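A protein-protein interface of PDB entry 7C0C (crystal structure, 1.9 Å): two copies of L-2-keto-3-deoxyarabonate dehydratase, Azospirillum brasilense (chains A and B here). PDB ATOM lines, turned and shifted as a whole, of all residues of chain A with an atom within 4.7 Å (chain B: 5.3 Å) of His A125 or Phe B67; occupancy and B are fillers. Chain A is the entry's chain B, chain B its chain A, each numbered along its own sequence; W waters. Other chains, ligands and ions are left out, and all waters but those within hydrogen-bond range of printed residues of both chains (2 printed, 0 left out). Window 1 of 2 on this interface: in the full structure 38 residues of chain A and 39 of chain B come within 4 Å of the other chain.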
ATOM      1  N   HIS A  97      20.332   9.873 -11.154  1.00  0.00           N
ATOM      2  CA  HIS A  97      21.773   9.827 -10.971  1.00  0.00           C
ATOM      3  C   HIS A  97      22.094   8.627 -10.097  1.00  0.00           C
ATOM      4  O   HIS A  97      21.253   8.172  -9.316  1.00  0.00           O
ATOM      5  CB  HIS A  97      22.319  11.115 -10.337  1.00  0.00           C
ATOM      6  CG  HIS A  97      23.781  11.334 -10.582  1.00  0.00           C
ATOM      7  ND1 HIS A  97      24.758  10.863  -9.730  1.00  0.00           N
ATOM      8  CD2 HIS A  97      24.431  11.971 -11.585  1.00  0.00           C
ATOM      9  CE1 HIS A  97      25.947  11.202 -10.197  1.00  0.00           C
ATOM     10  NE2 HIS A  97      25.777  11.875 -11.322  1.00  0.00           N
ATOM     11  N   TYR A  98      23.313   8.111 -10.243  1.00  0.00           N
ATOM     12  CA  TYR A  98      23.742   7.020  -9.379  1.00  0.00           C
ATOM     13  C   TYR A  98      23.802   7.471  -7.925  1.00  0.00           C
ATOM     14  O   TYR A  98      23.302   6.782  -7.031  1.00  0.00           O
ATOM     15  CB  TYR A  98      25.095   6.481  -9.841  1.00  0.00           C
ATOM     16  CG  TYR A  98      25.604   5.322  -9.013  1.00  0.00           C
ATOM     17  CD1 TYR A  98      26.416   5.538  -7.906  1.00  0.00           C
ATOM     18  CD2 TYR A  98      25.271   4.010  -9.336  1.00  0.00           C
ATOM     19  CE1 TYR A  98      26.882   4.486  -7.144  1.00  0.00           C
ATOM     20  CE2 TYR A  98      25.734   2.950  -8.578  1.00  0.00           C
ATOM     21  CZ  TYR A  98      26.543   3.195  -7.485  1.00  0.00           C
ATOM     22  OH  TYR A  98      27.010   2.153  -6.721  1.00  0.00           O
ATOM     23  N   SER A  99      24.392   8.642  -7.678  1.00  0.00           N
ATOM     24  CA  SER A  99      24.600   9.119  -6.314  1.00  0.00           C
ATOM     25  C   SER A  99      23.292   9.594  -5.686  1.00  0.00           C
ATOM     26  O   SER A  99      22.539  10.364  -6.293  1.00  0.00           O
ATOM     27  CB  SER A  99      25.623  10.253  -6.300  1.00  0.00           C
ATOM     28  OG  SER A  99      25.580  10.963  -5.071  1.00  0.00           O
ATOM     29  N   TYR A 124      22.045   3.259 -10.982  1.00  0.00           N
ATOM     30  CA  TYR A 124      22.728   2.279 -11.821  1.00  0.00           C
ATOM     31  C   TYR A 124      23.818   2.990 -12.606  1.00  0.00           C
ATOM     32  O   TYR A 124      23.865   4.222 -12.666  1.00  0.00           O
ATOM     33  CB  TYR A 124      21.759   1.581 -12.783  1.00  0.00           C
ATOM     34  CG  TYR A 124      21.251   2.490 -13.887  1.00  0.00           C
ATOM     35  CD1 TYR A 124      21.878   2.537 -15.132  1.00  0.00           C
ATOM     36  CD2 TYR A 124      20.152   3.309 -13.681  1.00  0.00           C
ATOM     37  CE1 TYR A 124      21.413   3.370 -16.140  1.00  0.00           C
ATOM     38  CE2 TYR A 124      19.679   4.146 -14.683  1.00  0.00           C
ATOM     39  CZ  TYR A 124      20.315   4.173 -15.908  1.00  0.00           C
ATOM     40  OH  TYR A 124      19.850   5.004 -16.898  1.00  0.00           O
ATOM     41  N   HIS A 125      24.690   2.198 -13.228  1.00  0.00           N
ATOM     42  CA  HIS A 125      25.575   2.730 -14.254  1.00  0.00           C
ATOM     43  C   HIS A 125      25.981   1.628 -15.216  1.00  0.00           C
ATOM     44  O   HIS A 125      26.344   0.526 -14.795  1.00  0.00           O
ATOM     45  CB  HIS A 125      26.840   3.366 -13.678  1.00  0.00           C
ATOM     46  CG  HIS A 125      27.806   3.807 -14.734  1.00  0.00           C
ATOM     47  ND1 HIS A 125      27.681   5.007 -15.399  1.00  0.00           N
ATOM     48  CD2 HIS A 125      28.889   3.194 -15.265  1.00  0.00           C
ATOM     49  CE1 HIS A 125      28.657   5.123 -16.280  1.00  0.00           C
ATOM     50  NE2 HIS A 125      29.404   4.036 -16.220  1.00  0.00           N
ATOM     51  N   GLY A 126      25.937   1.946 -16.506  1.00  0.00           N
ATOM     52  CA  GLY A 126      26.417   1.050 -17.533  1.00  0.00           C
ATOM     53  C   GLY A 126      25.672  -0.268 -17.547  1.00  0.00           C
ATOM     54  O   GLY A 126      24.470  -0.353 -17.266  1.00  0.00           O
ATOM     55  N   ALA A 127      26.405  -1.324 -17.888  1.00  0.00           N
ATOM     56  CA  ALA A 127      25.842  -2.660 -17.972  1.00  0.00           C
ATOM     57  C   ALA A 127      26.050  -3.478 -16.707  1.00  0.00           C
ATOM     58  O   ALA A 127      25.408  -4.522 -16.556  1.00  0.00           O
ATOM     59  CB  ALA A 127      26.448  -3.411 -19.166  1.00  0.00           C
ATOM     60  N   THR A 128      26.908  -3.026 -15.789  1.00  0.00           N
ATOM     61  CA  THR A 128      27.385  -3.878 -14.704  1.00  0.00           C
ATOM     62  C   THR A 128      27.217  -3.304 -13.302  1.00  0.00           C
ATOM     63  O   THR A 128      27.185  -4.088 -12.347  1.00  0.00           O
ATOM     64  CB  THR A 128      28.868  -4.218 -14.914  1.00  0.00           C
ATOM     65  OG1 THR A 128      29.626  -3.007 -15.005  1.00  0.00           O
ATOM     66  CG2 THR A 128      29.056  -5.016 -16.203  1.00  0.00           C
ATOM     67  N   PHE A 129      27.114  -1.989 -13.133  1.00  0.00           N
ATOM     68  CA  PHE A 129      27.053  -1.386 -11.803  1.00  0.00           C
ATOM     69  C   PHE A 129      25.599  -1.322 -11.348  1.00  0.00           C
ATOM     70  O   PHE A 129      24.822  -0.496 -11.837  1.00  0.00           O
ATOM     71  CB  PHE A 129      27.696  -0.002 -11.807  1.00  0.00           C
ATOM     72  CG  PHE A 129      29.181  -0.030 -12.032  1.00  0.00           C
ATOM     73  CD1 PHE A 129      30.052  -0.196 -10.969  1.00  0.00           C
ATOM     74  CD2 PHE A 129      29.706   0.097 -13.309  1.00  0.00           C
ATOM     75  CE1 PHE A 129      31.422  -0.229 -11.174  1.00  0.00           C
ATOM     76  CE2 PHE A 129      31.074   0.065 -13.521  1.00  0.00           C
ATOM     77  CZ  PHE A 129      31.933  -0.098 -12.452  1.00  0.00           C
ATOM     78  N   ARG A 130      25.237  -2.189 -10.407  1.00  0.00           N
ATOM     79  CA  ARG A 130      23.881  -2.279  -9.889  1.00  0.00           C
ATOM     80  C   ARG A 130      23.878  -2.058  -8.379  1.00  0.00           C
ATOM     81  O   ARG A 130      24.926  -1.990  -7.731  1.00  0.00           O
ATOM     82  CB  ARG A 130      23.248  -3.631 -10.238  1.00  0.00           C
ATOM     83  CG  ARG A 130      23.123  -3.881 -11.739  1.00  0.00           C
ATOM     84  CD  ARG A 130      22.234  -2.842 -12.406  1.00  0.00           C
ATOM     85  NE  ARG A 130      22.122  -3.071 -13.847  1.00  0.00           N
ATOM     86  CZ  ARG A 130      22.804  -2.396 -14.768  1.00  0.00           C
ATOM     87  NH1 ARG A 130      23.650  -1.438 -14.404  1.00  0.00           N
ATOM     88  NH2 ARG A 130      22.635  -2.677 -16.056  1.00  0.00           N
ATOM     89  N   ASN B  62      36.586   3.819 -13.120  1.00  0.00           N
ATOM     90  CA  ASN B  62      35.497   3.147 -12.416  1.00  0.00           C
ATOM     91  C   ASN B  62      35.834   2.922 -10.947  1.00  0.00           C
ATOM     92  O   ASN B  62      34.966   3.068 -10.075  1.00  0.00           O
ATOM     93  CB  ASN B  62      35.164   1.822 -13.103  1.00  0.00           C
ATOM     94  CG  ASN B  62      34.335   2.014 -14.359  1.00  0.00           C
ATOM     95  OD1 ASN B  62      33.579   2.981 -14.471  1.00  0.00           O
ATOM     96  ND2 ASN B  62      34.467   1.087 -15.311  1.00  0.00           N
ATOM     97  N   GLU B  65      34.964   5.667  -8.606  1.00  0.00           N
ATOM     98  CA  GLU B  65      33.536   5.968  -8.481  1.00  0.00           C
ATOM     99  C   GLU B  65      33.141   7.152  -9.363  1.00  0.00           C
ATOM    100  O   GLU B  65      32.391   8.037  -8.944  1.00  0.00           O
ATOM    101  CB  GLU B  65      33.147   6.220  -7.022  1.00  0.00           C
ATOM    102  CG  GLU B  65      33.246   4.988  -6.132  1.00  0.00           C
ATOM    103  CD  GLU B  65      33.141   5.322  -4.654  1.00  0.00           C
ATOM    104  OE1 GLU B  65      32.006   5.480  -4.151  1.00  0.00           O
ATOM    105  OE2 GLU B  65      34.197   5.428  -3.997  1.00  0.00           O
ATOM    106  N   GLN B  66      33.644   7.162 -10.602  1.00  0.00           N
ATOM    107  CA  GLN B  66      33.359   8.269 -11.515  1.00  0.00           C
ATOM    108  C   GLN B  66      31.865   8.435 -11.762  1.00  0.00           C
ATOM    109  O   GLN B  66      31.402   9.548 -12.034  1.00  0.00           O
ATOM    110  CB  GLN B  66      34.093   8.063 -12.842  1.00  0.00           C
ATOM    111  CG  GLN B  66      33.788   6.738 -13.533  1.00  0.00           C
ATOM    112  CD  GLN B  66      32.599   6.824 -14.468  1.00  0.00           C
ATOM    113  OE1 GLN B  66      32.134   7.916 -14.800  1.00  0.00           O
ATOM    114  NE2 GLN B  66      32.097   5.671 -14.896  1.00  0.00           N
ATOM    115  N   PHE B  67      31.095   7.349 -11.675  1.00  0.00           N
ATOM    116  CA  PHE B  67      29.658   7.423 -11.906  1.00  0.00           C
ATOM    117  C   PHE B  67      28.904   8.075 -10.752  1.00  0.00           C
ATOM    118  O   PHE B  67      27.725   8.405 -10.918  1.00  0.00           O
ATOM    119  CB  PHE B  67      29.103   6.021 -12.161  1.00  0.00           C
ATOM    120  CG  PHE B  67      29.681   4.973 -11.255  1.00  0.00           C
ATOM    121  CD1 PHE B  67      29.240   4.853  -9.949  1.00  0.00           C
ATOM    122  CD2 PHE B  67      30.678   4.124 -11.703  1.00  0.00           C
ATOM    123  CE1 PHE B  67      29.774   3.901  -9.109  1.00  0.00           C
ATOM    124  CE2 PHE B  67      31.217   3.169 -10.869  1.00  0.00           C
ATOM    125  CZ  PHE B  67      30.764   3.055  -9.570  1.00  0.00           C
ATOM    126  N   ALA B  68      29.544   8.267  -9.599  1.00  0.00           N
ATOM    127  CA  ALA B  68      28.898   8.849  -8.430  1.00  0.00           C
ATOM    128  C   ALA B  68      29.239  10.321  -8.226  1.00  0.00           C
ATOM    129  O   ALA B  68      28.858  10.895  -7.201  1.00  0.00           O
ATOM    130  CB  ALA B  68      29.266   8.053  -7.175  1.00  0.00           C
ATOM    131  N   ILE B  69      29.938  10.951  -9.171  1.00  0.00           N
ATOM    132  CA  ILE B  69      30.368  12.335  -9.015  1.00  0.00           C
ATOM    133  C   ILE B  69      29.796  13.177 -10.149  1.00  0.00           C
ATOM    134  O   ILE B  69      29.474  12.679 -11.231  1.00  0.00           O
ATOM    135  CB  ILE B  69      31.905  12.468  -8.963  1.00  0.00           C
ATOM    136  CG1 ILE B  69      32.534  11.957 -10.260  1.00  0.00           C
ATOM    137  CG2 ILE B  69      32.472  11.725  -7.754  1.00  0.00           C
ATOM    138  CD1 ILE B  69      34.001  12.307 -10.397  1.00  0.00           C
ATOM    139  N   TYR B 124      28.183   5.015 -24.635  1.00  0.00           N
ATOM    140  CA  TYR B 124      27.162   4.091 -24.161  1.00  0.00           C
ATOM    141  C   TYR B 124      26.354   4.774 -23.071  1.00  0.00           C
ATOM    142  O   TYR B 124      26.808   5.735 -22.444  1.00  0.00           O
ATOM    143  CB  TYR B 124      27.775   2.789 -23.619  1.00  0.00           C
ATOM    144  CG  TYR B 124      28.453   2.932 -22.265  1.00  0.00           C
ATOM    145  CD1 TYR B 124      29.807   3.226 -22.172  1.00  0.00           C
ATOM    146  CD2 TYR B 124      27.741   2.767 -21.081  1.00  0.00           C
ATOM    147  CE1 TYR B 124      30.432   3.356 -20.943  1.00  0.00           C
ATOM    148  CE2 TYR B 124      28.357   2.903 -19.847  1.00  0.00           C
ATOM    149  CZ  TYR B 124      29.702   3.195 -19.784  1.00  0.00           C
ATOM    150  OH  TYR B 124      30.320   3.326 -18.557  1.00  0.00           O
ATOM    151  N   GLY B 126      23.615   3.123 -19.873  1.00  0.00           N
ATOM    152  CA  GLY B 126      22.817   2.110 -19.224  1.00  0.00           C
ATOM    153  C   GLY B 126      22.939   0.753 -19.888  1.00  0.00           C
ATOM    154  O   GLY B 126      23.993   0.360 -20.402  1.00  0.00           O
ATOM    155  N   ALA B 158      31.622  -2.758 -18.422  1.00  0.00           N
ATOM    156  CA  ALA B 158      30.623  -1.786 -17.980  1.00  0.00           C
ATOM    157  C   ALA B 158      29.933  -1.102 -19.155  1.00  0.00           C
ATOM    158  O   ALA B 158      28.783  -0.671 -19.030  1.00  0.00           O
ATOM    159  CB  ALA B 158      31.263  -0.745 -17.062  1.00  0.00           C
ATOM    160  N   ILE B 271      35.928  -1.970  -5.403  1.00  0.00           N
ATOM    161  CA  ILE B 271      36.360  -0.575  -5.458  1.00  0.00           C
ATOM    162  C   ILE B 271      36.863  -0.109  -4.098  1.00  0.00           C
ATOM    163  O   ILE B 271      37.868   0.606  -3.997  1.00  0.00           O
ATOM    164  CB  ILE B 271      35.202   0.311  -5.959  1.00  0.00           C
ATOM    165  CG1 ILE B 271      34.863  -0.016  -7.410  1.00  0.00           C
ATOM    166  CG2 ILE B 271      35.526   1.790  -5.789  1.00  0.00           C
ATOM    167  CD1 ILE B 271      33.510   0.498  -7.844  1.00  0.00           C
ATOM    168  N   MET B 293      26.126   2.996  -3.096  1.00  0.00           N
ATOM    169  CA  MET B 293      27.054   1.878  -3.176  1.00  0.00           C
ATOM    170  C   MET B 293      27.176   1.252  -1.794  1.00  0.00           C
ATOM    171  O   MET B 293      27.495   1.965  -0.829  1.00  0.00           O
ATOM    172  CB  MET B 293      28.429   2.308  -3.677  1.00  0.00           C
ATOM    173  CG  MET B 293      29.433   1.163  -3.706  1.00  0.00           C
ATOM    174  SD  MET B 293      30.944   1.529  -4.611  1.00  0.00           S
ATOM    175  CE  MET B 293      30.268   2.082  -6.170  1.00  0.00           C
HETATM  176  O   HOH W   1      25.313   8.477 -12.454  1.00  0.00           O
HETATM  177  O   HOH W   2      25.066   4.264 -17.641  1.00  0.00           O
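Tyr A124 touches Gly B126, and with the chains exchanged Gly A126 touches Tyr B124.
Gly B126 touches its own counterpart, Gly A126.
Of the 21 pairs that touch across the chains among the printed residues, 3 have their exchanged pair printed and touching as well.
The backbone NH of Ser A99 lies within hydrogen-bond range of a ring nitrogen (ND1) of His A97.
The side-chain amide oxygen of Asn B62 sits at hydrogen-bond distance from the side-chain amide nitrogen of Gln B66, 3.1 Å away.
NH2 of Arg A130 is in hydrogen-bond range of O of Ala A127, 3.4 Å away.
NH1 of Arg A130 sits at hydrogen-bond distance from O of His A125 (3.4 Å).
The backbone carbonyl oxygen (O) of Gly A126 lies within hydrogen-bond range of the guanidinium group (NH1) of Arg A130 (3.2 Å).
Ala B68 touches His A97 (C to CE1, 3.9 Å).
O of Ile B69 touches NE2 of His A97, 3.8 Å away.
CB of Ala B68 touches CD1 of Tyr A98, 3.9 Å away.
CA of Gly B126 touches CE1 of Tyr A124, 3.6 Å away.
CG of His A125 touches CB of Phe B67 (3.6 Å).
Gly A126 touches Tyr B124.
Ala A127 touches Gly B126.
Thr A128 touches Ala B158 (OG1 to CA, 3.4 Å).
CE2 of Phe A129 touches CB of Ala B158, 3.6 Å away.
Ile B271 touches Phe A129 (CD1 to CE1, 3.997 Å).
Phe B67 touches just these residues of chain A: His A97, Tyr A98, His A125 and Phe A129.
Printed residues of chain A within 4 Å of Asn B62: Phe A129.
Of the printed residues of chain A, Ala B68 touches His A97 (3.9 Å), Tyr A98 (3.9 Å) and Ser A99 (3.4 Å).
Arg A130 touches none of the printed residues of chain B.
The nearest printed residue of chain B that does not touch Phe A129 is Met B293 (5.3 Å).
Water W2 bridges the backbone NH (N) of Gly A126 (2.7 Å) and the backbone NH (N) of Gly B126 (2.9 Å).
Water W1 lies within hydrogen-bond range of O of Phe B67 and N of Tyr A98.
O of Gly A126 lies close to O of Gly B126 (3.3 Å).
N of Ala A127 sits at hydrogen-bond distance from O of Ala B158.
The side-chain hydroxyl of Tyr B124 is in hydrogen-bond range of a ring nitrogen (NE2) of His A125, 2.6 Å away.
The side-chain amide nitrogen of Gln B66 is in hydrogen-bond range of a ring nitrogen (NE2) of His A125, at 3.4 Å.
Hydrophobic or aromatic side chains of chain A within 4 Å of the printed part of chain B: His A97, Tyr A98, Tyr A124, His A125, Ala A127 and Phe A129.
Printed residues of chain B that touch a printed residue of chain A: Asn B62, Gln B66, Phe B67, Ala B68, Ile B69, Tyr B124, Gly B126, Ala B158, Ile B271 and Met B293.
Hydrophobic or aromatic side chains of chain B that line the printed part of chain A: Phe B67, Ala B68, Tyr B124, Ala B158, Ile B271 and Met B293.
Among the printed residues, 21 pairs touch across the chains.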
